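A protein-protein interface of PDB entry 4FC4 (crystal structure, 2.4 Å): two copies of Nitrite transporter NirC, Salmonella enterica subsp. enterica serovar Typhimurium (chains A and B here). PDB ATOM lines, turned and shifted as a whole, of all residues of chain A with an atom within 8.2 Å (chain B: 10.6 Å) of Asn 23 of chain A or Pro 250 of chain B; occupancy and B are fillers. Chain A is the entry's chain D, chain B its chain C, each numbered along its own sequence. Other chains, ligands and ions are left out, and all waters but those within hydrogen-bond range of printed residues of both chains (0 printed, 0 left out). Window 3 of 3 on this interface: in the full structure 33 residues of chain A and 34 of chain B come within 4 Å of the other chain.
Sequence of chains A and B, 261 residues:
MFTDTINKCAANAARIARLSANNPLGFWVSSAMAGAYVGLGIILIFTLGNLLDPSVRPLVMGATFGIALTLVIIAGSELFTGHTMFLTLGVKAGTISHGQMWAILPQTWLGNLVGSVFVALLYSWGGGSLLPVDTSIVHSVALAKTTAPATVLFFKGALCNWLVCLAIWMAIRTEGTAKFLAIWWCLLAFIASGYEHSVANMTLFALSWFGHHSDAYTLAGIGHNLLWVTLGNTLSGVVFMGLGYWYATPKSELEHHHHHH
N of Gly 26 of chain A is in hydrogen-bond range of OD1 of Asn 23 of chain A.
OG1 of Thr 249 of chain B sits at hydrogen-bond distance from O of Trp 246 of chain B (3.4 Å).
Pro 250 of chain B touches Leu 19 of chain A.
O of Tyr 247 of chain B touches OD1 of Asn 23 of chain A, at 3.9 Å.
Thr 249 of chain B touches Asn 23 of chain A.
Asn 23 of chain A touches Pro 250 of chain B.
Tyr 247 of chain B touches Leu 25 of chain A (CD1 to CD2, 3.7 Å).
CA of Gly 26 of chain A touches O of Tyr 247 of chain B (3.1 Å).
CA of Gly 26 of chain A touches CA of Ala 248 of chain B (3.8 Å).
Gly 244 of chain B touches Val 29 of chain A (O to CG1, 3.4 Å).
Of the printed residues of chain B, Asn 23 of chain A touches Tyr 247, Thr 249 and Pro 250.
Pro 250 of chain B touches just these residues of chain A: Leu 19 and Asn 23.
No residue of chain B comes within 4 Å of Asn 22 of chain A.
No residue of chain B comes within 4 Å of Pro 24 of chain A.
Of the printed residues of chain A, Thr 249 of chain B touches Asn 23 (3.7 Å).
Printed residues of chain A within 4 Å of Ala 248 of chain B: Gly 26.
Printed residues of chain A within 4 Å of Tyr 247 of chain B: Asn 23, Leu 25 and Gly 26.
Printed residues of chain B within 4 Å of Val 29 of chain A: Gly 244.
Of the printed residues of chain A, Gly 244 of chain B touches Val 29.
Thr 3 of chain B touches none of the printed residues of chain A.
The nearest residue of chain B that does not touch Asn 23 of chain A is Ala 248 of chain B (5.1 Å).
The nearest residue of chain A that does not touch Pro 250 of chain B is Arg 18 of chain A (6.1 Å).
The nearest printed residue of chain A that does not touch Gly 244 of chain B is Ser 30 of chain A (6.2 Å).
Of the 13 printed residues of chain B, 5 touch a printed residue of chain A.
Of the 16 printed residues of chain A, 5 touch a printed residue of chain B.
No position is printed for both chains.
Of the 8 pairs that touch across the chains among the printed residues, none has its exchanged pair printed and touching as well.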
ATOM      1  N   ARG A  15     -17.956 -16.019  16.234  1.00  0.00           N
ATOM      2  CA  ARG A  15     -18.089 -15.130  17.421  1.00  0.00           C
ATOM      3  C   ARG A  15     -19.289 -15.494  18.325  1.00  0.00           C
ATOM      4  O   ARG A  15     -19.112 -15.639  19.557  1.00  0.00           O
ATOM      5  CB  ARG A  15     -18.112 -13.632  17.086  1.00  0.00           C
ATOM      6  CG  ARG A  15     -17.973 -12.748  18.329  1.00  0.00           C
ATOM      7  CD  ARG A  15     -18.258 -11.275  18.084  1.00  0.00           C
ATOM      8  NE  ARG A  15     -19.534 -11.047  17.379  1.00  0.00           N
ATOM      9  CZ  ARG A  15     -20.748 -11.154  17.920  1.00  0.00           C
ATOM     10  NH1 ARG A  15     -20.917 -11.515  19.190  1.00  0.00           N
ATOM     11  NH2 ARG A  15     -21.818 -10.952  17.177  1.00  0.00           N
ATOM     12  N   ILE A  16     -20.475 -15.625  17.713  1.00  0.00           N
ATOM     13  CA  ILE A  16     -21.684 -16.177  18.378  1.00  0.00           C
ATOM     14  C   ILE A  16     -21.387 -17.476  19.161  1.00  0.00           C
ATOM     15  O   ILE A  16     -21.764 -17.596  20.339  1.00  0.00           O
ATOM     16  CB  ILE A  16     -22.841 -16.421  17.367  1.00  0.00           C
ATOM     17  CG1 ILE A  16     -23.383 -15.105  16.831  1.00  0.00           C
ATOM     18  CG2 ILE A  16     -23.995 -17.186  17.999  1.00  0.00           C
ATOM     19  CD1 ILE A  16     -23.875 -15.222  15.406  1.00  0.00           C
ATOM     20  N   ALA A  17     -20.689 -18.418  18.523  1.00  0.00           N
ATOM     21  CA  ALA A  17     -20.294 -19.672  19.196  1.00  0.00           C
ATOM     22  C   ALA A  17     -19.399 -19.476  20.437  1.00  0.00           C
ATOM     23  O   ALA A  17     -19.665 -20.066  21.489  1.00  0.00           O
ATOM     24  CB  ALA A  17     -19.654 -20.647  18.211  1.00  0.00           C
ATOM     25  N   ARG A  18     -18.346 -18.655  20.316  1.00  0.00           N
ATOM     26  CA  ARG A  18     -17.422 -18.397  21.439  1.00  0.00           C
ATOM     27  C   ARG A  18     -18.192 -17.715  22.578  1.00  0.00           C
ATOM     28  O   ARG A  18     -17.993 -18.032  23.736  1.00  0.00           O
ATOM     29  CB  ARG A  18     -16.164 -17.595  21.012  1.00  0.00           C
ATOM     30  CG  ARG A  18     -15.174 -18.346  20.099  1.00  0.00           C
ATOM     31  CD  ARG A  18     -13.905 -17.560  19.756  1.00  0.00           C
ATOM     32  NE  ARG A  18     -14.184 -16.164  19.345  1.00  0.00           N
ATOM     33  CZ  ARG A  18     -14.123 -15.705  18.091  1.00  0.00           C
ATOM     34  NH1 ARG A  18     -14.405 -14.439  17.814  1.00  0.00           N
ATOM     35  NH2 ARG A  18     -13.797 -16.516  17.104  1.00  0.00           N
ATOM     36  N   LEU A  19     -19.109 -16.818  22.228  1.00  0.00           N
ATOM     37  CA  LEU A  19     -19.948 -16.179  23.214  1.00  0.00           C
ATOM     38  C   LEU A  19     -20.810 -17.245  23.922  1.00  0.00           C
ATOM     39  O   LEU A  19     -20.882 -17.284  25.161  1.00  0.00           O
ATOM     40  CB  LEU A  19     -20.797 -15.112  22.553  1.00  0.00           C
ATOM     41  CG  LEU A  19     -21.471 -14.102  23.479  1.00  0.00           C
ATOM     42  CD1 LEU A  19     -20.408 -13.239  24.162  1.00  0.00           C
ATOM     43  CD2 LEU A  19     -22.526 -13.256  22.742  1.00  0.00           C
ATOM     44  N   SER A  20     -21.412 -18.132  23.130  1.00  0.00           N
ATOM     45  CA  SER A  20     -22.290 -19.189  23.651  1.00  0.00           C
ATOM     46  C   SER A  20     -21.541 -20.122  24.619  1.00  0.00           C
ATOM     47  O   SER A  20     -22.027 -20.427  25.700  1.00  0.00           O
ATOM     48  CB  SER A  20     -22.913 -19.979  22.486  1.00  0.00           C
ATOM     49  OG  SER A  20     -23.791 -20.983  22.956  1.00  0.00           O
ATOM     50  N   ALA A  21     -20.331 -20.515  24.227  1.00  0.00           N
ATOM     51  CA  ALA A  21     -19.526 -21.488  24.938  1.00  0.00           C
ATOM     52  C   ALA A  21     -18.696 -20.898  26.097  1.00  0.00           C
ATOM     53  O   ALA A  21     -18.650 -21.470  27.187  1.00  0.00           O
ATOM     54  CB  ALA A  21     -18.633 -22.219  23.950  1.00  0.00           C
ATOM     55  N   ASN A  22     -18.048 -19.765  25.851  1.00  0.00           N
ATOM     56  CA  ASN A  22     -17.146 -19.120  26.810  1.00  0.00           C
ATOM     57  C   ASN A  22     -17.830 -18.090  27.705  1.00  0.00           C
ATOM     58  O   ASN A  22     -17.438 -17.922  28.851  1.00  0.00           O
ATOM     59  CB  ASN A  22     -15.964 -18.457  26.080  1.00  0.00           C
ATOM     60  CG  ASN A  22     -15.250 -19.412  25.116  1.00  0.00           C
ATOM     61  OD1 ASN A  22     -15.491 -20.609  25.127  1.00  0.00           O
ATOM     62  ND2 ASN A  22     -14.373 -18.873  24.275  1.00  0.00           N
ATOM     63  N   ASN A  23     -18.844 -17.392  27.190  1.00  0.00           N
ATOM     64  CA  ASN A  23     -19.515 -16.372  27.998  1.00  0.00           C
ATOM     65  C   ASN A  23     -21.043 -16.475  28.143  1.00  0.00           C
ATOM     66  O   ASN A  23     -21.761 -15.570  27.725  1.00  0.00           O
ATOM     67  CB  ASN A  23     -19.115 -14.973  27.542  1.00  0.00           C
ATOM     68  CG  ASN A  23     -19.043 -14.018  28.699  1.00  0.00           C
ATOM     69  OD1 ASN A  23     -20.036 -13.371  29.041  1.00  0.00           O
ATOM     70  ND2 ASN A  23     -17.886 -13.994  29.376  1.00  0.00           N
ATOM     71  N   PRO A  24     -21.535 -17.564  28.770  1.00  0.00           N
ATOM     72  CA  PRO A  24     -22.980 -17.838  28.871  1.00  0.00           C
ATOM     73  C   PRO A  24     -23.822 -16.631  29.327  1.00  0.00           C
ATOM     74  O   PRO A  24     -24.815 -16.307  28.685  1.00  0.00           O
ATOM     75  CB  PRO A  24     -23.059 -19.014  29.893  1.00  0.00           C
ATOM     76  CG  PRO A  24     -21.692 -19.174  30.460  1.00  0.00           C
ATOM     77  CD  PRO A  24     -20.738 -18.615  29.451  1.00  0.00           C
ATOM     78  N   LEU A  25     -23.412 -15.969  30.405  1.00  0.00           N
ATOM     79  CA  LEU A  25     -24.063 -14.761  30.892  1.00  0.00           C
ATOM     80  C   LEU A  25     -24.205 -13.711  29.773  1.00  0.00           C
ATOM     81  O   LEU A  25     -25.294 -13.165  29.557  1.00  0.00           O
ATOM     82  CB  LEU A  25     -23.273 -14.192  32.077  1.00  0.00           C
ATOM     83  CG  LEU A  25     -23.619 -12.853  32.742  1.00  0.00           C
ATOM     84  CD1 LEU A  25     -25.087 -12.748  33.146  1.00  0.00           C
ATOM     85  CD2 LEU A  25     -22.697 -12.640  33.929  1.00  0.00           C
ATOM     86  N   GLY A  26     -23.114 -13.467  29.045  1.00  0.00           N
ATOM     87  CA  GLY A  26     -23.084 -12.463  27.980  1.00  0.00           C
ATOM     88  C   GLY A  26     -24.051 -12.795  26.877  1.00  0.00           C
ATOM     89  O   GLY A  26     -24.749 -11.925  26.360  1.00  0.00           O
ATOM     90  N   PHE A  27     -24.120 -14.076  26.551  1.00  0.00           N
ATOM     91  CA  PHE A  27     -24.956 -14.541  25.465  1.00  0.00           C
ATOM     92  C   PHE A  27     -26.410 -14.299  25.799  1.00  0.00           C
ATOM     93  O   PHE A  27     -27.152 -13.775  24.964  1.00  0.00           O
ATOM     94  CB  PHE A  27     -24.714 -16.018  25.195  1.00  0.00           C
ATOM     95  CG  PHE A  27     -25.549 -16.570  24.098  1.00  0.00           C
ATOM     96  CD1 PHE A  27     -26.860 -16.963  24.333  1.00  0.00           C
ATOM     97  CD2 PHE A  27     -25.023 -16.723  22.832  1.00  0.00           C
ATOM     98  CE1 PHE A  27     -27.636 -17.502  23.329  1.00  0.00           C
ATOM     99  CE2 PHE A  27     -25.795 -17.260  21.810  1.00  0.00           C
ATOM    100  CZ  PHE A  27     -27.099 -17.649  22.063  1.00  0.00           C
ATOM    101  N   TRP A  28     -26.801 -14.671  27.015  1.00  0.00           N
ATOM    102  CA  TRP A  28     -28.193 -14.575  27.429  1.00  0.00           C
ATOM    103  C   TRP A  28     -28.677 -13.150  27.540  1.00  0.00           C
ATOM    104  O   TRP A  28     -29.798 -12.826  27.094  1.00  0.00           O
ATOM    105  CB  TRP A  28     -28.430 -15.365  28.709  1.00  0.00           C
ATOM    106  CG  TRP A  28     -28.514 -16.845  28.433  1.00  0.00           C
ATOM    107  CD1 TRP A  28     -27.527 -17.808  28.647  1.00  0.00           C
ATOM    108  CD2 TRP A  28     -29.631 -17.577  27.822  1.00  0.00           C
ATOM    109  NE1 TRP A  28     -27.953 -19.048  28.252  1.00  0.00           N
ATOM    110  CE2 TRP A  28     -29.200 -18.993  27.749  1.00  0.00           C
ATOM    111  CE3 TRP A  28     -30.904 -17.231  27.379  1.00  0.00           C
ATOM    112  CZ2 TRP A  28     -30.026 -19.998  27.237  1.00  0.00           C
ATOM    113  CZ3 TRP A  28     -31.736 -18.248  26.872  1.00  0.00           C
ATOM    114  CH2 TRP A  28     -31.305 -19.601  26.802  1.00  0.00           C
ATOM    115  N   VAL A  29     -27.835 -12.297  28.128  1.00  0.00           N
ATOM    116  CA  VAL A  29     -28.122 -10.872  28.220  1.00  0.00           C
ATOM    117  C   VAL A  29     -28.291 -10.334  26.802  1.00  0.00           C
ATOM    118  O   VAL A  29     -29.314  -9.732  26.457  1.00  0.00           O
ATOM    119  CB  VAL A  29     -27.017 -10.151  29.015  1.00  0.00           C
ATOM    120  CG1 VAL A  29     -27.207  -8.647  29.004  1.00  0.00           C
ATOM    121  CG2 VAL A  29     -27.018 -10.672  30.451  1.00  0.00           C
ATOM    122  N   SER A  30     -27.324 -10.643  25.951  1.00  0.00           N
ATOM    123  CA  SER A  30     -27.347 -10.189  24.577  1.00  0.00           C
ATOM    124  C   SER A  30     -28.543 -10.716  23.746  1.00  0.00           C
ATOM    125  O   SER A  30     -29.029 -10.012  22.866  1.00  0.00           O
ATOM    126  CB  SER A  30     -26.004 -10.519  23.922  1.00  0.00           C
ATOM    127  OG  SER A  30     -25.755  -9.673  22.817  1.00  0.00           O
ATOM    128  N   MET B   1     -15.855  -2.095  19.459  1.00  0.00           N
ATOM    129  CA  MET B   1     -16.702  -3.248  19.915  1.00  0.00           C
ATOM    130  C   MET B   1     -17.618  -2.827  21.097  1.00  0.00           C
ATOM    131  O   MET B   1     -17.952  -1.626  21.222  1.00  0.00           O
ATOM    132  CB  MET B   1     -15.840  -4.499  20.228  1.00  0.00           C
ATOM    133  CG  MET B   1     -14.392  -4.282  20.686  1.00  0.00           C
ATOM    134  SD  MET B   1     -13.718  -5.768  21.507  1.00  0.00           S
ATOM    135  CE  MET B   1     -11.931  -5.531  21.599  1.00  0.00           C
ATOM    136  N   PHE B   2     -18.039  -3.787  21.946  1.00  0.00           N
ATOM    137  CA  PHE B   2     -18.637  -3.421  23.255  1.00  0.00           C
ATOM    138  C   PHE B   2     -17.588  -2.787  24.214  1.00  0.00           C
ATOM    139  O   PHE B   2     -17.848  -1.725  24.794  1.00  0.00           O
ATOM    140  CB  PHE B   2     -19.395  -4.585  23.944  1.00  0.00           C
ATOM    141  CG  PHE B   2     -20.726  -4.969  23.300  1.00  0.00           C
ATOM    142  CD1 PHE B   2     -21.446  -4.079  22.483  1.00  0.00           C
ATOM    143  CD2 PHE B   2     -21.271  -6.237  23.534  1.00  0.00           C
ATOM    144  CE1 PHE B   2     -22.661  -4.462  21.903  1.00  0.00           C
ATOM    145  CE2 PHE B   2     -22.476  -6.624  22.959  1.00  0.00           C
ATOM    146  CZ  PHE B   2     -23.179  -5.738  22.153  1.00  0.00           C
ATOM    147  N   THR B   3     -16.414  -3.415  24.369  1.00  0.00           N
ATOM    148  CA  THR B   3     -15.343  -2.855  25.233  1.00  0.00           C
ATOM    149  C   THR B   3     -14.915  -1.409  24.854  1.00  0.00           C
ATOM    150  O   THR B   3     -14.739  -0.577  25.740  1.00  0.00           O
ATOM    151  CB  THR B   3     -14.109  -3.803  25.480  1.00  0.00           C
ATOM    152  OG1 THR B   3     -14.132  -4.932  24.590  1.00  0.00           O
ATOM    153  CG2 THR B   3     -14.088  -4.318  26.947  1.00  0.00           C
ATOM    154  N   ASP B   4     -14.771  -1.115  23.560  1.00  0.00           N
ATOM    155  CA  ASP B   4     -14.476   0.239  23.087  1.00  0.00           C
ATOM    156  C   ASP B   4     -15.528   1.242  23.533  1.00  0.00           C
ATOM    157  O   ASP B   4     -15.199   2.322  24.056  1.00  0.00           O
ATOM    158  CB  ASP B   4     -14.422   0.265  21.557  1.00  0.00           C
ATOM    159  CG  ASP B   4     -13.015   0.090  21.021  1.00  0.00           C
ATOM    160  OD1 ASP B   4     -12.355  -0.948  21.325  1.00  0.00           O
ATOM    161  OD2 ASP B   4     -12.569   0.997  20.292  1.00  0.00           O
ATOM    162  N   ILE B   6     -17.646   0.940  25.986  1.00  0.00           N
ATOM    163  CA  ILE B   6     -17.631   1.005  27.436  1.00  0.00           C
ATOM    164  C   ILE B   6     -16.503   1.932  27.919  1.00  0.00           C
ATOM    165  O   ILE B   6     -16.768   2.868  28.677  1.00  0.00           O
ATOM    166  CB  ILE B   6     -17.602  -0.411  28.078  1.00  0.00           C
ATOM    167  CG1 ILE B   6     -18.997  -1.041  27.988  1.00  0.00           C
ATOM    168  CG2 ILE B   6     -17.084  -0.384  29.527  1.00  0.00           C
ATOM    169  CD1 ILE B   6     -18.981  -2.549  28.164  1.00  0.00           C
ATOM    170  N   LEU B 243     -25.072  -1.783  33.470  1.00  0.00           N
ATOM    171  CA  LEU B 243     -24.783  -3.178  33.813  1.00  0.00           C
ATOM    172  C   LEU B 243     -25.051  -4.166  32.662  1.00  0.00           C
ATOM    173  O   LEU B 243     -24.225  -5.029  32.351  1.00  0.00           O
ATOM    174  CB  LEU B 243     -25.549  -3.566  35.080  1.00  0.00           C
ATOM    175  CG  LEU B 243     -25.158  -2.831  36.378  1.00  0.00           C
ATOM    176  CD1 LEU B 243     -26.060  -3.322  37.492  1.00  0.00           C
ATOM    177  CD2 LEU B 243     -23.685  -3.040  36.785  1.00  0.00           C
ATOM    178  N   GLY B 244     -26.206  -4.023  32.024  1.00  0.00           N
ATOM    179  CA  GLY B 244     -26.558  -4.817  30.845  1.00  0.00           C
ATOM    180  C   GLY B 244     -25.436  -4.961  29.835  1.00  0.00           C
ATOM    181  O   GLY B 244     -25.048  -6.090  29.494  1.00  0.00           O
ATOM    182  N   TYR B 245     -24.899  -3.846  29.335  1.00  0.00           N
ATOM    183  CA  TYR B 245     -23.751  -3.984  28.410  1.00  0.00           C
ATOM    184  C   TYR B 245     -22.440  -4.473  29.044  1.00  0.00           C
ATOM    185  O   TYR B 245     -21.675  -5.227  28.401  1.00  0.00           O
ATOM    186  CB  TYR B 245     -23.546  -2.771  27.490  1.00  0.00           C
ATOM    187  CG  TYR B 245     -24.488  -2.805  26.300  1.00  0.00           C
ATOM    188  CD1 TYR B 245     -24.289  -3.702  25.249  1.00  0.00           C
ATOM    189  CD2 TYR B 245     -25.626  -1.986  26.263  1.00  0.00           C
ATOM    190  CE1 TYR B 245     -25.183  -3.764  24.179  1.00  0.00           C
ATOM    191  CE2 TYR B 245     -26.519  -2.032  25.203  1.00  0.00           C
ATOM    192  CZ  TYR B 245     -26.294  -2.920  24.163  1.00  0.00           C
ATOM    193  OH  TYR B 245     -27.161  -2.927  23.098  1.00  0.00           O
ATOM    194  N   TRP B 246     -22.198  -4.095  30.300  1.00  0.00           N
ATOM    195  CA  TRP B 246     -21.055  -4.636  31.044  1.00  0.00           C
ATOM    196  C   TRP B 246     -21.034  -6.151  31.025  1.00  0.00           C
ATOM    197  O   TRP B 246     -20.005  -6.736  30.677  1.00  0.00           O
ATOM    198  CB  TRP B 246     -21.030  -4.078  32.458  1.00  0.00           C
ATOM    199  CG  TRP B 246     -19.826  -4.457  33.268  1.00  0.00           C
ATOM    200  CD1 TRP B 246     -19.759  -5.412  34.285  1.00  0.00           C
ATOM    201  CD2 TRP B 246     -18.475  -3.867  33.200  1.00  0.00           C
ATOM    202  NE1 TRP B 246     -18.500  -5.464  34.808  1.00  0.00           N
ATOM    203  CE2 TRP B 246     -17.676  -4.565  34.208  1.00  0.00           C
ATOM    204  CE3 TRP B 246     -17.875  -2.891  32.429  1.00  0.00           C
ATOM    205  CZ2 TRP B 246     -16.313  -4.277  34.418  1.00  0.00           C
ATOM    206  CZ3 TRP B 246     -16.498  -2.622  32.637  1.00  0.00           C
ATOM    207  CH2 TRP B 246     -15.746  -3.283  33.628  1.00  0.00           C
ATOM    208  N   TYR B 247     -22.164  -6.802  31.308  1.00  0.00           N
ATOM    209  CA  TYR B 247     -22.210  -8.272  31.294  1.00  0.00           C
ATOM    210  C   TYR B 247     -22.326  -8.971  29.917  1.00  0.00           C
ATOM    211  O   TYR B 247     -22.136 -10.190  29.804  1.00  0.00           O
ATOM    212  CB  TYR B 247     -23.236  -8.787  32.309  1.00  0.00           C
ATOM    213  CG  TYR B 247     -22.832  -8.414  33.715  1.00  0.00           C
ATOM    214  CD1 TYR B 247     -21.825  -9.108  34.381  1.00  0.00           C
ATOM    215  CD2 TYR B 247     -23.415  -7.334  34.356  1.00  0.00           C
ATOM    216  CE1 TYR B 247     -21.435  -8.751  35.663  1.00  0.00           C
ATOM    217  CE2 TYR B 247     -23.039  -6.966  35.633  1.00  0.00           C
ATOM    218  CZ  TYR B 247     -22.053  -7.666  36.284  1.00  0.00           C
ATOM    219  OH  TYR B 247     -21.690  -7.276  37.562  1.00  0.00           O
ATOM    220  N   ALA B 248     -22.608  -8.188  28.882  1.00  0.00           N
ATOM    221  CA  ALA B 248     -22.730  -8.698  27.519  1.00  0.00           C
ATOM    222  C   ALA B 248     -21.366  -8.908  26.847  1.00  0.00           C
ATOM    223  O   ALA B 248     -21.275  -9.585  25.812  1.00  0.00           O
ATOM    224  CB  ALA B 248     -23.621  -7.774  26.676  1.00  0.00           C
ATOM    225  N   THR B 249     -20.308  -8.341  27.427  1.00  0.00           N
ATOM    226  CA  THR B 249     -18.974  -8.453  26.819  1.00  0.00           C
ATOM    227  C   THR B 249     -18.229  -9.722  27.220  1.00  0.00           C
ATOM    228  O   THR B 249     -18.296 -10.148  28.376  1.00  0.00           O
ATOM    229  CB  THR B 249     -18.064  -7.277  27.188  1.00  0.00           C
ATOM    230  OG1 THR B 249     -17.537  -7.493  28.494  1.00  0.00           O
ATOM    231  CG2 THR B 249     -18.818  -5.961  27.146  1.00  0.00           C
ATOM    232  N   PRO B 250     -17.508 -10.330  26.267  1.00  0.00           N
ATOM    233  CA  PRO B 250     -16.673 -11.468  26.661  1.00  0.00           C
ATOM    234  C   PRO B 250     -15.289 -11.010  27.125  1.00  0.00           C
ATOM    235  O   PRO B 250     -15.175 -10.406  28.190  1.00  0.00           O
ATOM    236  CB  PRO B 250     -16.593 -12.328  25.378  1.00  0.00           C
ATOM    237  CG  PRO B 250     -17.501 -11.664  24.374  1.00  0.00           C
ATOM    238  CD  PRO B 250     -17.631 -10.231  24.803  1.00  0.00           C
